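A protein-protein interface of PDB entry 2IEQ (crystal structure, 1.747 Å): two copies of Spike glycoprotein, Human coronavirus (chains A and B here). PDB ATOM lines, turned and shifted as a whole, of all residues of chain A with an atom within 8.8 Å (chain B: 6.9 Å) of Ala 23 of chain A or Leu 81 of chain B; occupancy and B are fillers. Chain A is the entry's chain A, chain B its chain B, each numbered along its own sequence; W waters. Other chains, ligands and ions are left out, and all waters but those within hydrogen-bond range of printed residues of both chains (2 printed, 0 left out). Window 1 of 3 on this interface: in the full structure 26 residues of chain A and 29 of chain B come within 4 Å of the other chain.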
ATOM      1  N   ALA A  16      19.844  11.656  23.692  1.00  0.00           N
ATOM      2  CA  ALA A  16      18.939  12.175  22.653  1.00  0.00           C
ATOM      3  C   ALA A  16      17.508  11.663  22.918  1.00  0.00           C
ATOM      4  O   ALA A  16      16.527  12.411  22.785  1.00  0.00           O
ATOM      5  CB  ALA A  16      19.451  11.679  21.285  1.00  0.00           C
ATOM      6  N   ILE A  17      17.383  10.419  23.385  1.00  0.00           N
ATOM      7  CA  ILE A  17      16.046   9.862  23.619  1.00  0.00           C
ATOM      8  C   ILE A  17      15.395  10.643  24.782  1.00  0.00           C
ATOM      9  O   ILE A  17      14.249  11.012  24.692  1.00  0.00           O
ATOM     10  CB  ILE A  17      16.103   8.330  23.885  1.00  0.00           C
ATOM     11  CG1 ILE A  17      16.536   7.626  22.594  1.00  0.00           C
ATOM     12  CG2 ILE A  17      14.717   7.818  24.281  1.00  0.00           C
ATOM     13  CD1 ILE A  17      16.998   6.204  22.740  1.00  0.00           C
ATOM     14  N   THR A  18      16.175  10.904  25.841  1.00  0.00           N
ATOM     15  CA  THR A  18      15.735  11.733  26.974  1.00  0.00           C
ATOM     16  C   THR A  18      15.253  13.103  26.514  1.00  0.00           C
ATOM     17  O   THR A  18      14.151  13.540  26.885  1.00  0.00           O
ATOM     18  CB  THR A  18      16.867  11.851  28.022  1.00  0.00           C
ATOM     19  OG1 THR A  18      17.217  10.537  28.477  1.00  0.00           O
ATOM     20  CG2 THR A  18      16.384  12.738  29.192  1.00  0.00           C
ATOM     21  N   GLN A  19      16.029  13.776  25.671  1.00  0.00           N
ATOM     22  CA  GLN A  19      15.733  15.111  25.190  1.00  0.00           C
ATOM     23  C   GLN A  19      14.445  15.073  24.360  1.00  0.00           C
ATOM     24  O   GLN A  19      13.591  15.981  24.423  1.00  0.00           O
ATOM     25  CB  GLN A  19      16.875  15.579  24.274  1.00  0.00           C
ATOM     26  CG  GLN A  19      18.231  16.020  24.978  1.00  0.00           C
ATOM     27  CD  GLN A  19      19.275  16.311  23.880  1.00  0.00           C
ATOM     28  OE1 GLN A  19      19.061  17.227  23.042  1.00  0.00           O
ATOM     29  NE2 GLN A  19      20.348  15.496  23.809  1.00  0.00           N
ATOM     30  N   THR A  20      14.283  14.020  23.590  1.00  0.00           N
ATOM     31  CA  THR A  20      13.075  13.873  22.739  1.00  0.00           C
ATOM     32  C   THR A  20      11.831  13.687  23.621  1.00  0.00           C
ATOM     33  O   THR A  20      10.804  14.249  23.346  1.00  0.00           O
ATOM     34  CB  THR A  20      13.238  12.647  21.823  1.00  0.00           C
ATOM     35  OG1 THR A  20      14.404  12.812  21.000  1.00  0.00           O
ATOM     36  CG2 THR A  20      11.953  12.377  20.941  1.00  0.00           C
ATOM     37  N   ALA A  21      11.947  12.892  24.687  1.00  0.00           N
ATOM     38  CA  ALA A  21      10.803  12.637  25.556  1.00  0.00           C
ATOM     39  C   ALA A  21      10.405  13.958  26.177  1.00  0.00           C
ATOM     40  O   ALA A  21       9.213  14.259  26.265  1.00  0.00           O
ATOM     41  CB  ALA A  21      11.195  11.593  26.671  1.00  0.00           C
ATOM     42  N   GLU A  22      11.420  14.718  26.615  1.00  0.00           N
ATOM     43  CA  GLU A  22      11.209  16.025  27.237  1.00  0.00           C
ATOM     44  C   GLU A  22      10.558  17.007  26.259  1.00  0.00           C
ATOM     45  O   GLU A  22       9.598  17.744  26.594  1.00  0.00           O
ATOM     46  CB  GLU A  22      12.565  16.539  27.720  1.00  0.00           C
ATOM     47  CG  GLU A  22      13.003  15.820  29.029  1.00  0.00           C
ATOM     48  CD  GLU A  22      14.414  16.215  29.465  1.00  0.00           C
ATOM     49  OE1 GLU A  22      15.208  16.670  28.621  1.00  0.00           O
ATOM     50  OE2 GLU A  22      14.752  16.035  30.654  1.00  0.00           O
ATOM     51  N   ALA A  23      11.045  16.967  25.026  1.00  0.00           N
ATOM     52  CA  ALA A  23      10.513  17.858  23.999  1.00  0.00           C
ATOM     53  C   ALA A  23       9.070  17.494  23.735  1.00  0.00           C
ATOM     54  O   ALA A  23       8.193  18.375  23.636  1.00  0.00           O
ATOM     55  CB  ALA A  23      11.317  17.699  22.738  1.00  0.00           C
ATOM     56  N   ILE A  24       8.769  16.206  23.619  1.00  0.00           N
ATOM     57  CA  ILE A  24       7.325  15.851  23.422  1.00  0.00           C
ATOM     58  C   ILE A  24       6.422  16.289  24.601  1.00  0.00           C
ATOM     59  O   ILE A  24       5.238  16.734  24.427  1.00  0.00           O
ATOM     60  CB  ILE A  24       7.208  14.329  23.137  1.00  0.00           C
ATOM     61  CG1 ILE A  24       7.823  14.022  21.746  1.00  0.00           C
ATOM     62  CG2 ILE A  24       5.709  13.893  23.273  1.00  0.00           C
ATOM     63  CD1 ILE A  24       8.109  12.513  21.478  1.00  0.00           C
ATOM     64  N   HIS A  25       6.967  16.141  25.825  1.00  0.00           N
ATOM     65  CA  HIS A  25       6.268  16.662  27.016  1.00  0.00           C
ATOM     66  C   HIS A  25       5.924  18.149  26.821  1.00  0.00           C
ATOM     67  O   HIS A  25       4.767  18.540  27.037  1.00  0.00           O
ATOM     68  CB  HIS A  25       7.104  16.461  28.288  1.00  0.00           C
ATOM     69  CG  HIS A  25       6.406  16.966  29.516  1.00  0.00           C
ATOM     70  ND1 HIS A  25       6.889  18.015  30.264  1.00  0.00           N
ATOM     71  CD2 HIS A  25       5.221  16.609  30.071  1.00  0.00           C
ATOM     72  CE1 HIS A  25       6.042  18.273  31.250  1.00  0.00           C
ATOM     73  NE2 HIS A  25       5.028  17.428  31.163  1.00  0.00           N
ATOM     74  N   THR A  26       6.899  18.963  26.396  1.00  0.00           N
ATOM     75  CA  THR A  26       6.690  20.425  26.213  1.00  0.00           C
ATOM     76  C   THR A  26       5.619  20.685  25.128  1.00  0.00           C
ATOM     77  O   THR A  26       4.747  21.560  25.262  1.00  0.00           O
ATOM     78  CB  THR A  26       8.049  21.120  25.838  1.00  0.00           C
ATOM     79  OG1 THR A  26       8.983  20.961  26.925  1.00  0.00           O
ATOM     80  CG2 THR A  26       7.872  22.636  25.597  1.00  0.00           C
ATOM     81  N   VAL A  27       5.696  19.926  24.042  1.00  0.00           N
ATOM     82  CA  VAL A  27       4.682  20.084  22.965  1.00  0.00           C
ATOM     83  C   VAL A  27       3.273  19.776  23.558  1.00  0.00           C
ATOM     84  O   VAL A  27       2.293  20.447  23.234  1.00  0.00           O
ATOM     85  CB  VAL A  27       4.945  19.118  21.774  1.00  0.00           C
ATOM     86  CG1 VAL A  27       3.780  19.231  20.807  1.00  0.00           C
ATOM     87  CG2 VAL A  27       6.235  19.529  21.035  1.00  0.00           C
ATOM     88  N   THR A  28       3.165  18.764  24.416  1.00  0.00           N
ATOM     89  CA  THR A  28       1.875  18.373  25.039  1.00  0.00           C
ATOM     90  C   THR A  28       1.309  19.548  25.876  1.00  0.00           C
ATOM     91  O   THR A  28       0.092  19.893  25.799  1.00  0.00           O
ATOM     92  CB  THR A  28       2.044  17.097  25.927  1.00  0.00           C
ATOM     93  OG1 THR A  28       2.557  16.006  25.121  1.00  0.00           O
ATOM     94  CG2 THR A  28       0.719  16.677  26.449  1.00  0.00           C
ATOM     95  N   ILE A  29       2.195  20.172  26.644  1.00  0.00           N
ATOM     96  CA  ILE A  29       1.824  21.321  27.469  1.00  0.00           C
ATOM     97  C   ILE A  29       1.363  22.471  26.521  1.00  0.00           C
ATOM     98  O   ILE A  29       0.293  23.055  26.756  1.00  0.00           O
ATOM     99  CB  ILE A  29       3.001  21.825  28.319  1.00  0.00           C
ATOM    100  CG1 ILE A  29       3.244  20.855  29.468  1.00  0.00           C
ATOM    101  CG2 ILE A  29       2.663  23.269  28.894  1.00  0.00           C
ATOM    102  CD1 ILE A  29       4.549  21.097  30.198  1.00  0.00           C
ATOM    103  N   ALA A  30       2.117  22.711  25.450  1.00  0.00           N
ATOM    104  CA  ALA A  30       1.759  23.775  24.462  1.00  0.00           C
ATOM    105  C   ALA A  30       0.375  23.516  23.861  1.00  0.00           C
ATOM    106  O   ALA A  30      -0.507  24.420  23.818  1.00  0.00           O
ATOM    107  CB  ALA A  30       2.795  23.874  23.391  1.00  0.00           C
ATOM    108  N   LEU A  31       0.153  22.284  23.396  1.00  0.00           N
ATOM    109  CA  LEU A  31      -1.114  21.919  22.739  1.00  0.00           C
ATOM    110  C   LEU A  31      -2.327  22.066  23.727  1.00  0.00           C
ATOM    111  O   LEU A  31      -3.395  22.527  23.317  1.00  0.00           O
ATOM    112  CB  LEU A  31      -1.070  20.475  22.228  1.00  0.00           C
ATOM    113  CG  LEU A  31      -0.044  20.265  21.082  1.00  0.00           C
ATOM    114  CD1 LEU A  31       0.097  18.763  20.843  1.00  0.00           C
ATOM    115  CD2 LEU A  31      -0.498  21.023  19.771  1.00  0.00           C
ATOM    116  N   LEU A  81       0.202  11.461  23.389  1.00  0.00           N
ATOM    117  CA  LEU A  81       1.535  12.063  23.530  1.00  0.00           C
ATOM    118  C   LEU A  81       2.080  11.804  24.925  1.00  0.00           C
ATOM    119  O   LEU A  81       3.280  11.541  25.074  1.00  0.00           O
ATOM    120  CB  LEU A  81       1.550  13.572  23.237  1.00  0.00           C
ATOM    121  CG  LEU A  81       1.269  13.915  21.748  1.00  0.00           C
ATOM    122  CD1 LEU A  81       1.075  15.394  21.621  1.00  0.00           C
ATOM    123  CD2 LEU A  81       2.332  13.326  20.745  1.00  0.00           C
ATOM    124  N   THR A  85       5.616   9.913  25.687  1.00  0.00           N
ATOM    125  CA  THR A  85       6.587  10.468  26.606  1.00  0.00           C
ATOM    126  C   THR A  85       7.027   9.444  27.657  1.00  0.00           C
ATOM    127  O   THR A  85       8.222   9.176  27.885  1.00  0.00           O
ATOM    128  CB  THR A  85       6.019  11.723  27.342  1.00  0.00           C
ATOM    129  OG1 THR A  85       5.802  12.779  26.365  1.00  0.00           O
ATOM    130  CG2 THR A  85       7.031  12.230  28.378  1.00  0.00           C
ATOM    131  N   LEU A  88       8.980   6.487  26.042  1.00  0.00           N
ATOM    132  CA  LEU A  88      10.330   6.942  25.723  1.00  0.00           C
ATOM    133  C   LEU A  88      11.184   6.960  26.990  1.00  0.00           C
ATOM    134  O   LEU A  88      12.314   6.460  26.971  1.00  0.00           O
ATOM    135  CB  LEU A  88      10.348   8.340  25.083  1.00  0.00           C
ATOM    136  CG  LEU A  88       9.968   8.367  23.579  1.00  0.00           C
ATOM    137  CD1 LEU A  88       9.665   9.816  23.118  1.00  0.00           C
ATOM    138  CD2 LEU A  88      11.049   7.644  22.653  1.00  0.00           C
ATOM    139  N   PHE A  89      10.654   7.545  28.080  1.00  0.00           N
ATOM    140  CA  PHE A  89      11.408   7.483  29.366  1.00  0.00           C
ATOM    141  C   PHE A  89      11.701   6.039  29.822  1.00  0.00           C
ATOM    142  O   PHE A  89      12.805   5.737  30.289  1.00  0.00           O
ATOM    143  CB  PHE A  89      10.679   8.250  30.443  1.00  0.00           C
ATOM    144  CG  PHE A  89      10.887   9.753  30.371  1.00  0.00           C
ATOM    145  CD1 PHE A  89      12.176  10.328  30.246  1.00  0.00           C
ATOM    146  CD2 PHE A  89       9.794  10.606  30.442  1.00  0.00           C
ATOM    147  CE1 PHE A  89      12.340  11.711  30.192  1.00  0.00           C
ATOM    148  CE2 PHE A  89       9.942  11.977  30.370  1.00  0.00           C
ATOM    149  CZ  PHE A  89      11.233  12.538  30.255  1.00  0.00           C
ATOM    150  N   THR B  20      14.709  14.147  13.988  1.00  0.00           N
ATOM    151  CA  THR B  20      13.933  14.491  15.173  1.00  0.00           C
ATOM    152  C   THR B  20      14.162  15.972  15.551  1.00  0.00           C
ATOM    153  O   THR B  20      13.221  16.688  15.814  1.00  0.00           O
ATOM    154  CB  THR B  20      14.300  13.604  16.383  1.00  0.00           C
ATOM    155  OG1 THR B  20      14.031  12.259  16.072  1.00  0.00           O
ATOM    156  CG2 THR B  20      13.431  13.966  17.605  1.00  0.00           C
ATOM    157  N   ALA B  21      15.411  16.439  15.506  1.00  0.00           N
ATOM    158  CA  ALA B  21      15.667  17.831  15.806  1.00  0.00           C
ATOM    159  C   ALA B  21      14.958  18.732  14.789  1.00  0.00           C
ATOM    160  O   ALA B  21      14.390  19.727  15.169  1.00  0.00           O
ATOM    161  CB  ALA B  21      17.139  18.098  15.777  1.00  0.00           C
ATOM    162  N   ILE B  24      11.216  18.757  15.562  1.00  0.00           N
ATOM    163  CA  ILE B  24      10.946  19.715  16.670  1.00  0.00           C
ATOM    164  C   ILE B  24      11.014  21.177  16.248  1.00  0.00           C
ATOM    165  O   ILE B  24      10.185  21.967  16.621  1.00  0.00           O
ATOM    166  CB  ILE B  24      11.905  19.447  17.863  1.00  0.00           C
ATOM    167  CG1 ILE B  24      11.651  18.032  18.419  1.00  0.00           C
ATOM    168  CG2 ILE B  24      11.810  20.563  18.981  1.00  0.00           C
ATOM    169  CD1 ILE B  24      10.242  17.645  18.655  1.00  0.00           C
ATOM    170  N   HIS B  25      12.029  21.537  15.461  1.00  0.00           N
ATOM    171  CA  HIS B  25      12.113  22.898  14.916  1.00  0.00           C
ATOM    172  C   HIS B  25      10.848  23.283  14.102  1.00  0.00           C
ATOM    173  O   HIS B  25      10.306  24.378  14.282  1.00  0.00           O
ATOM    174  CB  HIS B  25      13.349  23.030  14.025  1.00  0.00           C
ATOM    175  CG  HIS B  25      13.376  24.325  13.264  1.00  0.00           C
ATOM    176  ND1 HIS B  25      13.319  24.369  11.888  1.00  0.00           N
ATOM    177  CD2 HIS B  25      13.417  25.606  13.686  1.00  0.00           C
ATOM    178  CE1 HIS B  25      13.320  25.630  11.488  1.00  0.00           C
ATOM    179  NE2 HIS B  25      13.411  26.399  12.552  1.00  0.00           N
ATOM    180  N   VAL B  27       7.859  21.940  14.491  1.00  0.00           N
ATOM    181  CA  VAL B  27       6.730  22.092  15.433  1.00  0.00           C
ATOM    182  C   VAL B  27       6.823  23.469  16.087  1.00  0.00           C
ATOM    183  O   VAL B  27       5.802  24.102  16.304  1.00  0.00           O
ATOM    184  CB  VAL B  27       6.729  20.951  16.480  1.00  0.00           C
ATOM    185  CG1 VAL B  27       5.622  21.238  17.562  1.00  0.00           C
ATOM    186  CG2 VAL B  27       6.444  19.593  15.777  1.00  0.00           C
ATOM    187  N   THR B  28       8.032  23.917  16.452  1.00  0.00           N
ATOM    188  CA  THR B  28       8.196  25.238  17.079  1.00  0.00           C
ATOM    189  C   THR B  28       7.620  26.362  16.169  1.00  0.00           C
ATOM    190  O   THR B  28       6.939  27.284  16.655  1.00  0.00           O
ATOM    191  CB  THR B  28       9.699  25.489  17.350  1.00  0.00           C
ATOM    192  OG1 THR B  28      10.146  24.450  18.243  1.00  0.00           O
ATOM    193  CG2 THR B  28       9.922  26.817  18.027  1.00  0.00           C
ATOM    194  N   LEU B  31       3.731  26.137  16.199  1.00  0.00           N
ATOM    195  CA  LEU B  31       3.182  26.633  17.480  1.00  0.00           C
ATOM    196  C   LEU B  31       3.300  28.175  17.587  1.00  0.00           C
ATOM    197  O   LEU B  31       2.386  28.830  18.140  1.00  0.00           O
ATOM    198  CB  LEU B  31       3.945  26.018  18.656  1.00  0.00           C
ATOM    199  CG  LEU B  31       3.789  24.508  18.846  1.00  0.00           C
ATOM    200  CD1 LEU B  31       4.834  24.075  19.909  1.00  0.00           C
ATOM    201  CD2 LEU B  31       2.326  24.156  19.321  1.00  0.00           C
ATOM    202  N   SER B  76       7.403  30.165  27.156  1.00  0.00           N
ATOM    203  CA  SER B  76       8.310  29.255  27.909  1.00  0.00           C
ATOM    204  C   SER B  76       8.453  27.961  27.122  1.00  0.00           C
ATOM    205  O   SER B  76       9.547  27.403  26.998  1.00  0.00           O
ATOM    206  CB  SER B  76       7.786  28.949  29.316  1.00  0.00           C
ATOM    207  OG  SER B  76       7.621  30.204  30.063  1.00  0.00           O
ATOM    208  N   GLU B  77       7.323  27.521  26.555  1.00  0.00           N
ATOM    209  CA  GLU B  77       7.342  26.287  25.744  1.00  0.00           C
ATOM    210  C   GLU B  77       8.184  26.456  24.513  1.00  0.00           C
ATOM    211  O   GLU B  77       8.959  25.530  24.145  1.00  0.00           O
ATOM    212  CB  GLU B  77       5.911  25.850  25.411  1.00  0.00           C
ATOM    213  CG  GLU B  77       5.088  25.390  26.637  1.00  0.00           C
ATOM    214  CD  GLU B  77       4.489  26.538  27.456  1.00  0.00           C
ATOM    215  OE1 GLU B  77       4.429  27.687  26.986  1.00  0.00           O
ATOM    216  OE2 GLU B  77       4.116  26.290  28.610  1.00  0.00           O
ATOM    217  N   LEU B  78       8.070  27.605  23.847  1.00  0.00           N
ATOM    218  CA  LEU B  78       8.847  27.887  22.619  1.00  0.00           C
ATOM    219  C   LEU B  78      10.323  27.898  22.897  1.00  0.00           C
ATOM    220  O   LEU B  78      11.143  27.292  22.146  1.00  0.00           O
ATOM    221  CB  LEU B  78       8.392  29.150  21.890  1.00  0.00           C
ATOM    222  CG  LEU B  78       6.958  29.084  21.331  1.00  0.00           C
ATOM    223  CD1 LEU B  78       6.543  30.454  20.886  1.00  0.00           C
ATOM    224  CD2 LEU B  78       6.782  28.105  20.137  1.00  0.00           C
ATOM    225  N   LYS B  79      10.662  28.507  24.031  1.00  0.00           N
ATOM    226  CA  LYS B  79      12.074  28.555  24.415  1.00  0.00           C
ATOM    227  C   LYS B  79      12.621  27.191  24.743  1.00  0.00           C
ATOM    228  O   LYS B  79      13.735  26.877  24.353  1.00  0.00           O
ATOM    229  CB  LYS B  79      12.284  29.526  25.567  1.00  0.00           C
ATOM    230  CG  LYS B  79      12.433  31.002  25.051  1.00  0.00           C
ATOM    231  CD  LYS B  79      11.466  31.296  23.899  1.00  0.00           C
ATOM    232  CE  LYS B  79      10.751  32.641  23.996  1.00  0.00           C
ATOM    233  NZ  LYS B  79       9.567  32.598  23.102  1.00  0.00           N
ATOM    234  N   GLN B  80      11.838  26.387  25.452  1.00  0.00           N
ATOM    235  CA  GLN B  80      12.229  25.034  25.795  1.00  0.00           C
ATOM    236  C   GLN B  80      12.433  24.212  24.524  1.00  0.00           C
ATOM    237  O   GLN B  80      13.391  23.478  24.457  1.00  0.00           O
ATOM    238  CB  GLN B  80      11.188  24.348  26.683  1.00  0.00           C
ATOM    239  CG  GLN B  80      11.153  24.891  28.124  1.00  0.00           C
ATOM    240  CD  GLN B  80      10.059  24.234  28.955  1.00  0.00           C
ATOM    241  OE1 GLN B  80       8.913  24.068  28.495  1.00  0.00           O
ATOM    242  NE2 GLN B  80      10.412  23.822  30.179  1.00  0.00           N
ATOM    243  N   LEU B  81      11.498  24.287  23.562  1.00  0.00           N
ATOM    244  CA  LEU B  81      11.691  23.604  22.250  1.00  0.00           C
ATOM    245  C   LEU B  81      12.909  24.047  21.456  1.00  0.00           C
ATOM    246  O   LEU B  81      13.618  23.211  20.864  1.00  0.00           O
ATOM    247  CB  LEU B  81      10.417  23.669  21.382  1.00  0.00           C
ATOM    248  CG  LEU B  81       9.216  22.958  22.041  1.00  0.00           C
ATOM    249  CD1 LEU B  81       7.964  23.258  21.196  1.00  0.00           C
ATOM    250  CD2 LEU B  81       9.411  21.412  22.243  1.00  0.00           C
ATOM    251  N   GLU B  82      13.182  25.353  21.449  1.00  0.00           N
ATOM    252  CA  GLU B  82      14.369  25.872  20.804  1.00  0.00           C
ATOM    253  C   GLU B  82      15.620  25.294  21.506  1.00  0.00           C
ATOM    254  O   GLU B  82      16.575  24.880  20.803  1.00  0.00           O
ATOM    255  CB  GLU B  82      14.359  27.411  20.780  1.00  0.00           C
ATOM    256  CG  GLU B  82      13.296  27.972  19.821  1.00  0.00           C
ATOM    257  CD  GLU B  82      12.707  29.317  20.308  1.00  0.00           C
ATOM    258  OE1 GLU B  82      13.387  30.033  21.091  1.00  0.00           O
ATOM    259  OE2 GLU B  82      11.555  29.648  19.915  1.00  0.00           O
ATOM    260  N   ALA B  83      15.589  25.208  22.840  1.00  0.00           N
ATOM    261  CA  ALA B  83      16.743  24.592  23.572  1.00  0.00           C
ATOM    262  C   ALA B  83      16.929  23.134  23.174  1.00  0.00           C
ATOM    263  O   ALA B  83      18.078  22.678  23.000  1.00  0.00           O
ATOM    264  CB  ALA B  83      16.619  24.728  25.062  1.00  0.00           C
ATOM    265  N   LYS B  84      15.812  22.399  23.065  1.00  0.00           N
ATOM    266  CA  LYS B  84      15.866  20.986  22.622  1.00  0.00           C
ATOM    267  C   LYS B  84      16.337  20.820  21.197  1.00  0.00           C
ATOM    268  O   LYS B  84      17.093  19.875  20.902  1.00  0.00           O
ATOM    269  CB  LYS B  84      14.524  20.267  22.829  1.00  0.00           C
ATOM    270  CG  LYS B  84      14.152  20.157  24.324  1.00  0.00           C
ATOM    271  CD  LYS B  84      14.975  19.110  25.058  1.00  0.00           C
ATOM    272  CE  LYS B  84      14.726  19.231  26.556  1.00  0.00           C
ATOM    273  NZ  LYS B  84      15.649  20.217  27.206  1.00  0.00           N
ATOM    274  N   THR B  85      15.893  21.675  20.285  1.00  0.00           N
ATOM    275  CA  THR B  85      16.427  21.643  18.931  1.00  0.00           C
ATOM    276  C   THR B  85      17.962  21.726  18.945  1.00  0.00           C
ATOM    277  O   THR B  85      18.664  20.898  18.344  1.00  0.00           O
ATOM    278  CB  THR B  85      15.790  22.750  18.083  1.00  0.00           C
ATOM    279  OG1 THR B  85      14.361  22.497  18.035  1.00  0.00           O
ATOM    280  CG2 THR B  85      16.376  22.752  16.683  1.00  0.00           C
ATOM    281  N   ALA B  86      18.467  22.743  19.650  1.00  0.00           N
ATOM    282  CA  ALA B  86      19.909  22.976  19.784  1.00  0.00           C
ATOM    283  C   ALA B  86      20.638  21.762  20.399  1.00  0.00           C
ATOM    284  O   ALA B  86      21.697  21.322  19.893  1.00  0.00           O
ATOM    285  CB  ALA B  86      20.122  24.188  20.633  1.00  0.00           C
ATOM    286  N   SER B  87      20.073  21.212  21.455  1.00  0.00           N
ATOM    287  CA  SER B  87      20.790  20.116  22.143  1.00  0.00           C
ATOM    288  C   SER B  87      20.786  18.853  21.344  1.00  0.00           C
ATOM    289  O   SER B  87      21.765  18.090  21.380  1.00  0.00           O
ATOM    290  CB  SER B  87      20.285  19.883  23.557  1.00  0.00           C
ATOM    291  OG  SER B  87      18.906  19.588  23.642  1.00  0.00           O
ATOM    292  N   LEU B  88      19.675  18.600  20.638  1.00  0.00           N
ATOM    293  CA  LEU B  88      19.622  17.387  19.820  1.00  0.00           C
ATOM    294  C   LEU B  88      20.647  17.548  18.699  1.00  0.00           C
ATOM    295  O   LEU B  88      21.346  16.589  18.328  1.00  0.00           O
ATOM    296  CB  LEU B  88      18.201  17.202  19.231  1.00  0.00           C
ATOM    297  CG  LEU B  88      17.150  16.608  20.186  1.00  0.00           C
ATOM    298  CD1 LEU B  88      15.746  16.816  19.635  1.00  0.00           C
ATOM    299  CD2 LEU B  88      17.416  15.089  20.518  1.00  0.00           C
HETATM  300  O   HOH W   1      15.086  19.431  29.769  1.00  0.00           O
HETATM  301  O   HOH W   2       7.742  22.240  29.545  1.00  0.00           O
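The side-chain hydroxyl (OG) of Ser 87 of chain B lies within hydrogen-bond range of the side-chain amide oxygen (OE1) of Gln 19 of chain A, at 2.4 Å.
The side-chain amide oxygen (OE1) of Gln 19 of chain A is in hydrogen-bond range of the backbone NH (N) of Leu 88 of chain B.
OE1 of Glu 22 of chain A is in salt-bridge range of NZ of Lys 84 of chain B (3.8 Å).
OE1 of Gln 80 of chain B sits close to OG1 of Thr 26 of chain A (3.5 Å).
The backbone carbonyl oxygen of Ala 83 of chain B sits at hydrogen-bond distance from the side-chain hydroxyl of Ser 87 of chain B.
The backbone carbonyl oxygen (O) of Ala 16 of chain A sits at hydrogen-bond distance from the side-chain hydroxyl (OG1) of Thr 20 of chain A.
The backbone carbonyl oxygen (O) of Lys 84 of chain B sits at hydrogen-bond distance from the side-chain hydroxyl (OG) of Ser 87 of chain B, 3.3 Å away.
O of Glu 22 of chain A lies within hydrogen-bond range of OG1 of Thr 26 of chain A (3.3 Å).
Leu 88 of chain B touches Ala 16 of chain A.
CD of Lys 84 of chain B touches O of Gln 19 of chain A, 3.5 Å away.
Thr 20 of chain A touches Thr 20 of chain B.
Thr 20 of chain A touches Leu 88 of chain B (OG1 to CD2, 3.8 Å).
CD2 of Leu 81 of chain B touches O of Ala 23 of chain A, at 3.6 Å.
Glu 77 of chain B touches Thr 26 of chain A (O to CG2, 3.4 Å).
Leu 81 of chain B touches Thr 26 of chain A.
Val 27 of chain A touches Leu 81 of chain B.
OE2 of Glu 77 of chain B touches CG2 of Ile 29 of chain A, at 3.4 Å.
Ala 23 of chain A touches just one residue of chain B: Leu 81.
Of chain A, only Ala 23, Thr 26 and Val 27 come within 4 Å of Leu 81 of chain B.
Printed residues of chain A within 4 Å of Gln 80 of chain B: Thr 26.
Of the printed residues of chain A, Glu 77 of chain B touches Thr 26 (3.4 Å) and Ile 29 (3.4 Å).
Of the printed residues of chain B, Thr 20 of chain A touches Thr 20 (3.7 Å) and Leu 88 (3.8 Å).
Leu 31 of chain B touches none of the printed residues of chain A.
Ala 86 of chain B touches none of the printed residues of chain A.
The nearest residue of chain B that does not touch Ala 23 of chain A is Lys 84 of chain B (4.1 Å).
The nearest residue of chain A that does not touch Leu 81 of chain B is Ile 24 of chain A (5.4 Å).
Hydrophobic or aromatic side chains of chain B within 4 Å of the printed part of chain A: Val 27, Leu 81 and Leu 88.
Printed residues of chain A that touch a printed residue of chain B: Ala 16, Gln 19, Thr 20, Glu 22, Ala 23, Thr 26, Val 27 and Ile 29.
Hydrophobic or aromatic side chains of chain A that line the printed part of chain B: Val 27 and Ile 29.
Along chain A the printed residues that touch a printed residue of chain B span positions 16 to 29.
Among the printed residues, Asp or Glu carboxylates within 4 Å of a Lys or Arg side-chain nitrogen of the other chain: Glu 22 of chain A with Lys 84 of chain B (3.8 Å).
Thr 20 of chain B touches its own counterpart, Thr 20 of chain A.
Thr 20 of chain A touches Leu 88 of chain B, but with the chains exchanged Leu 88 of chain A does not touch Thr 20 of chain B (7.9 Å).
Val 27 of chain B touches its own counterpart, Val 27 of chain A.
Val 27 of chain A touches Leu 81 of chain B, but with the chains exchanged Leu 81 of chain A does not touch Val 27 of chain B (8.4 Å).
Of the 14 pairs that touch across the chains among the printed residues, 2 have their exchanged pair printed and touching as well.
Water W2 bridges OE1 of Gln 80 of chain B and OG1 of Thr 26 of chain A.
Water W1 lies within hydrogen-bond range of the side-chain amino group (NZ) of Lys 84 of chain B and the side-chain carboxylate (OE1) of Glu 22 of chain A.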
